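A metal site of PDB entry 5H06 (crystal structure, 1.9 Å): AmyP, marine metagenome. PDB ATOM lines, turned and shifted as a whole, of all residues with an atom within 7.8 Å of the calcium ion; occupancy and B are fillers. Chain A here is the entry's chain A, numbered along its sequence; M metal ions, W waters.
The side-chain hydroxyl of Tyr 352 lies within hydrogen-bond range of the guanidinium group of Arg 308, 2.7 Å away.
Five residues have an atom within 4 Å of the calcium ion: Asp 304, Gln 307, Glu 348, Leu 349 and Tyr 352.
The calcium ion is bound by OE1 of Glu 348 (2.3 Å). The calcium ion is bound by O of Leu 349, at 2.3 Å. The calcium ion is bound by the side-chain amide oxygen (OE1) of Gln 307, at 2.3 Å. OD1 of Asp 304 is bound to the calcium ion (2.3 Å). O of Tyr 352 is bound to the calcium ion. Water W1 is bound to the calcium ion, 2.4 Å away. The calcium ion has six donor atoms within binding distance.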
ATOM      1  N   ARG A 301      20.629  -1.067  -0.119  1.00  0.00           N
ATOM      2  CA  ARG A 301      20.024  -1.975  -1.085  1.00  0.00           C
ATOM      3  C   ARG A 301      19.719  -3.326  -0.457  1.00  0.00           C
ATOM      4  O   ARG A 301      20.483  -3.822   0.376  1.00  0.00           O
ATOM      5  CB  ARG A 301      20.933  -2.166  -2.306  1.00  0.00           C
ATOM      6  CG  ARG A 301      20.887  -0.993  -3.286  1.00  0.00           C
ATOM      7  CD  ARG A 301      21.629  -1.331  -4.596  1.00  0.00           C
ATOM      8  NE  ARG A 301      21.544  -0.226  -5.557  1.00  0.00           N
ATOM      9  CZ  ARG A 301      20.448   0.075  -6.261  1.00  0.00           C
ATOM     10  NH1 ARG A 301      20.464   1.103  -7.103  1.00  0.00           N
ATOM     11  NH2 ARG A 301      19.350  -0.656  -6.124  1.00  0.00           N
ATOM     12  N   GLY A 303      19.982  -6.295  -1.610  1.00  0.00           N
ATOM     13  CA  GLY A 303      21.055  -7.275  -1.802  1.00  0.00           C
ATOM     14  C   GLY A 303      22.264  -7.036  -0.924  1.00  0.00           C
ATOM     15  O   GLY A 303      22.958  -7.991  -0.536  1.00  0.00           O
ATOM     16  N   ASP A 304      22.559  -5.780  -0.616  1.00  0.00           N
ATOM     17  CA  ASP A 304      23.619  -5.514   0.355  1.00  0.00           C
ATOM     18  C   ASP A 304      23.184  -5.874   1.763  1.00  0.00           C
ATOM     19  O   ASP A 304      24.012  -6.325   2.570  1.00  0.00           O
ATOM     20  CB  ASP A 304      24.071  -4.055   0.261  1.00  0.00           C
ATOM     21  CG  ASP A 304      24.869  -3.772  -0.997  1.00  0.00           C
ATOM     22  OD1 ASP A 304      25.728  -4.609  -1.342  1.00  0.00           O
ATOM     23  OD2 ASP A 304      24.644  -2.728  -1.656  1.00  0.00           O
ATOM     24  N   LEU A 305      21.895  -5.687   2.080  1.00  0.00           N
ATOM     25  CA  LEU A 305      21.384  -6.159   3.365  1.00  0.00           C
ATOM     26  C   LEU A 305      21.534  -7.659   3.506  1.00  0.00           C
ATOM     27  O   LEU A 305      21.807  -8.164   4.601  1.00  0.00           O
ATOM     28  CB  LEU A 305      19.909  -5.772   3.545  1.00  0.00           C
ATOM     29  CG  LEU A 305      19.674  -4.279   3.792  1.00  0.00           C
ATOM     30  CD1 LEU A 305      18.187  -3.956   3.782  1.00  0.00           C
ATOM     31  CD2 LEU A 305      20.342  -3.855   5.121  1.00  0.00           C
ATOM     32  N   GLN A 307      23.910  -9.501   2.181  1.00  0.00           N
ATOM     33  CA  GLN A 307      25.311  -9.768   2.450  1.00  0.00           C
ATOM     34  C   GLN A 307      25.703  -9.304   3.853  1.00  0.00           C
ATOM     35  O   GLN A 307      26.486  -9.965   4.542  1.00  0.00           O
ATOM     36  CB  GLN A 307      26.186  -9.080   1.392  1.00  0.00           C
ATOM     37  CG  GLN A 307      26.038  -9.648  -0.015  1.00  0.00           C
ATOM     38  CD  GLN A 307      26.824  -8.853  -1.046  1.00  0.00           C
ATOM     39  OE1 GLN A 307      26.697  -7.628  -1.146  1.00  0.00           O
ATOM     40  NE2 GLN A 307      27.640  -9.557  -1.827  1.00  0.00           N
ATOM     41  N   ARG A 308      25.171  -8.153   4.276  1.00  0.00           N
ATOM     42  CA  ARG A 308      25.482  -7.616   5.591  1.00  0.00           C
ATOM     43  C   ARG A 308      25.087  -8.586   6.692  1.00  0.00           C
ATOM     44  O   ARG A 308      25.797  -8.740   7.695  1.00  0.00           O
ATOM     45  CB  ARG A 308      24.787  -6.268   5.803  1.00  0.00           C
ATOM     46  CG  ARG A 308      24.886  -5.749   7.235  1.00  0.00           C
ATOM     47  CD  ARG A 308      24.240  -4.356   7.413  1.00  0.00           C
ATOM     48  NE  ARG A 308      24.894  -3.346   6.570  1.00  0.00           N
ATOM     49  CZ  ARG A 308      24.644  -2.045   6.652  1.00  0.00           C
ATOM     50  NH1 ARG A 308      25.278  -1.195   5.841  1.00  0.00           N
ATOM     51  NH2 ARG A 308      23.771  -1.575   7.549  1.00  0.00           N
ATOM     52  N   SER A 313      24.679 -13.988  -0.975  1.00  0.00           N
ATOM     53  CA  SER A 313      25.367 -13.108  -1.899  1.00  0.00           C
ATOM     54  C   SER A 313      25.023 -13.558  -3.318  1.00  0.00           C
ATOM     55  O   SER A 313      24.539 -14.683  -3.497  1.00  0.00           O
ATOM     56  CB  SER A 313      26.884 -13.121  -1.671  1.00  0.00           C
ATOM     57  OG  SER A 313      27.446 -14.394  -1.929  1.00  0.00           O
ATOM     58  N   PRO A 314      25.245 -12.707  -4.329  1.00  0.00           N
ATOM     59  CA  PRO A 314      24.712 -13.005  -5.676  1.00  0.00           C
ATOM     60  C   PRO A 314      25.190 -14.325  -6.270  1.00  0.00           C
ATOM     61  O   PRO A 314      24.545 -14.821  -7.208  1.00  0.00           O
ATOM     62  CB  PRO A 314      25.208 -11.817  -6.518  1.00  0.00           C
ATOM     63  CG  PRO A 314      25.345 -10.713  -5.542  1.00  0.00           C
ATOM     64  CD  PRO A 314      25.842 -11.355  -4.287  1.00  0.00           C
ATOM     65  N   TYR A 319      20.077 -15.991  -2.700  1.00  0.00           N
ATOM     66  CA  TYR A 319      20.053 -14.547  -2.893  1.00  0.00           C
ATOM     67  C   TYR A 319      18.906 -14.126  -3.814  1.00  0.00           C
ATOM     68  O   TYR A 319      18.181 -13.170  -3.517  1.00  0.00           O
ATOM     69  CB  TYR A 319      21.387 -14.102  -3.483  1.00  0.00           C
ATOM     70  CG  TYR A 319      21.557 -12.623  -3.777  1.00  0.00           C
ATOM     71  CD1 TYR A 319      21.211 -12.101  -5.017  1.00  0.00           C
ATOM     72  CD2 TYR A 319      22.101 -11.756  -2.828  1.00  0.00           C
ATOM     73  CE1 TYR A 319      21.393 -10.746  -5.310  1.00  0.00           C
ATOM     74  CE2 TYR A 319      22.274 -10.404  -3.110  1.00  0.00           C
ATOM     75  CZ  TYR A 319      21.922  -9.908  -4.343  1.00  0.00           C
ATOM     76  OH  TYR A 319      22.099  -8.569  -4.642  1.00  0.00           O
ATOM     77  N   ASP A 347      20.464  -5.572  -7.650  1.00  0.00           N
ATOM     78  CA  ASP A 347      21.666  -4.751  -7.525  1.00  0.00           C
ATOM     79  C   ASP A 347      22.254  -4.800  -6.119  1.00  0.00           C
ATOM     80  O   ASP A 347      21.557  -5.000  -5.125  1.00  0.00           O
ATOM     81  CB  ASP A 347      21.366  -3.285  -7.878  1.00  0.00           C
ATOM     82  CG  ASP A 347      21.733  -2.937  -9.311  1.00  0.00           C
ATOM     83  OD1 ASP A 347      22.317  -3.796 -10.000  1.00  0.00           O
ATOM     84  OD2 ASP A 347      21.452  -1.803  -9.753  1.00  0.00           O
ATOM     85  N   GLU A 348      23.566  -4.604  -6.042  1.00  0.00           N
ATOM     86  CA  GLU A 348      24.291  -4.534  -4.787  1.00  0.00           C
ATOM     87  C   GLU A 348      25.646  -3.927  -5.100  1.00  0.00           C
ATOM     88  O   GLU A 348      26.181  -4.109  -6.182  1.00  0.00           O
ATOM     89  CB  GLU A 348      24.429  -5.916  -4.118  1.00  0.00           C
ATOM     90  CG  GLU A 348      25.081  -7.013  -4.975  1.00  0.00           C
ATOM     91  CD  GLU A 348      26.615  -6.978  -4.937  1.00  0.00           C
ATOM     92  OE1 GLU A 348      27.186  -6.458  -3.960  1.00  0.00           O
ATOM     93  OE2 GLU A 348      27.254  -7.481  -5.877  1.00  0.00           O
ATOM     94  N   LEU A 349      26.169  -3.169  -4.153  1.00  0.00           N
ATOM     95  CA  LEU A 349      27.433  -2.482  -4.347  1.00  0.00           C
ATOM     96  C   LEU A 349      28.583  -3.469  -4.157  1.00  0.00           C
ATOM     97  O   LEU A 349      28.774  -4.012  -3.060  1.00  0.00           O
ATOM     98  CB  LEU A 349      27.551  -1.308  -3.379  1.00  0.00           C
ATOM     99  CG  LEU A 349      28.852  -0.521  -3.446  1.00  0.00           C
ATOM    100  CD1 LEU A 349      29.131  -0.057  -4.874  1.00  0.00           C
ATOM    101  CD2 LEU A 349      28.795   0.653  -2.480  1.00  0.00           C
ATOM    102  N   GLU A 350      29.337  -3.706  -5.225  1.00  0.00           N
ATOM    103  CA  GLU A 350      30.506  -4.577  -5.149  1.00  0.00           C
ATOM    104  C   GLU A 350      31.505  -4.059  -4.118  1.00  0.00           C
ATOM    105  O   GLU A 350      31.785  -2.853  -4.034  1.00  0.00           O
ATOM    106  CB  GLU A 350      31.176  -4.685  -6.516  1.00  0.00           C
ATOM    107  CG  GLU A 350      32.583  -5.258  -6.447  1.00  0.00           C
ATOM    108  CD  GLU A 350      33.342  -5.130  -7.756  1.00  0.00           C
ATOM    109  OE1 GLU A 350      32.686  -5.030  -8.820  1.00  0.00           O
ATOM    110  OE2 GLU A 350      34.595  -5.112  -7.721  1.00  0.00           O
ATOM    111  N   GLY A 351      32.046  -4.974  -3.321  1.00  0.00           N
ATOM    112  CA  GLY A 351      33.043  -4.610  -2.332  1.00  0.00           C
ATOM    113  C   GLY A 351      32.482  -4.029  -1.063  1.00  0.00           C
ATOM    114  O   GLY A 351      33.259  -3.623  -0.189  1.00  0.00           O
ATOM    115  N   TYR A 352      31.156  -3.999  -0.910  1.00  0.00           N
ATOM    116  CA  TYR A 352      30.510  -3.338   0.207  1.00  0.00           C
ATOM    117  C   TYR A 352      29.431  -4.236   0.801  1.00  0.00           C
ATOM    118  O   TYR A 352      28.713  -4.909   0.057  1.00  0.00           O
ATOM    119  CB  TYR A 352      29.863  -2.013  -0.250  1.00  0.00           C
ATOM    120  CG  TYR A 352      28.943  -1.429   0.795  1.00  0.00           C
ATOM    121  CD1 TYR A 352      29.440  -0.651   1.842  1.00  0.00           C
ATOM    122  CD2 TYR A 352      27.575  -1.697   0.760  1.00  0.00           C
ATOM    123  CE1 TYR A 352      28.596  -0.146   2.811  1.00  0.00           C
ATOM    124  CE2 TYR A 352      26.728  -1.207   1.723  1.00  0.00           C
ATOM    125  CZ  TYR A 352      27.240  -0.427   2.738  1.00  0.00           C
ATOM    126  OH  TYR A 352      26.397   0.049   3.684  1.00  0.00           O
ATOM    127  N   ALA A 353      29.308  -4.248   2.124  1.00  0.00           N
ATOM    128  CA  ALA A 353      28.133  -4.862   2.751  1.00  0.00           C
ATOM    129  C   ALA A 353      27.969  -4.371   4.181  1.00  0.00           C
ATOM    130  O   ALA A 353      26.917  -3.825   4.549  1.00  0.00           O
ATOM    131  CB  ALA A 353      28.221  -6.388   2.736  1.00  0.00           C
ATOM    132  N   GLN A 354      28.998  -4.578   4.999  1.00  0.00           N
ATOM    133  CA  GLN A 354      28.968  -4.138   6.374  1.00  0.00           C
ATOM    134  C   GLN A 354      28.861  -2.622   6.445  1.00  0.00           C
ATOM    135  O   GLN A 354      29.318  -1.899   5.551  1.00  0.00           O
ATOM    136  CB  GLN A 354      30.220  -4.620   7.120  1.00  0.00           C
ATOM    137  CG  GLN A 354      30.231  -6.112   7.348  1.00  0.00           C
ATOM    138  CD  GLN A 354      29.204  -6.539   8.385  1.00  0.00           C
ATOM    139  OE1 GLN A 354      29.205  -6.031   9.514  1.00  0.00           O
ATOM    140  NE2 GLN A 354      28.331  -7.469   8.016  1.00  0.00           N
HETATM  141 CA    CA M   1      27.706  -5.685  -1.889  1.00  0.00          CA
HETATM  142  O   HOH W   1      29.766  -6.801  -1.704  1.00  0.00           O
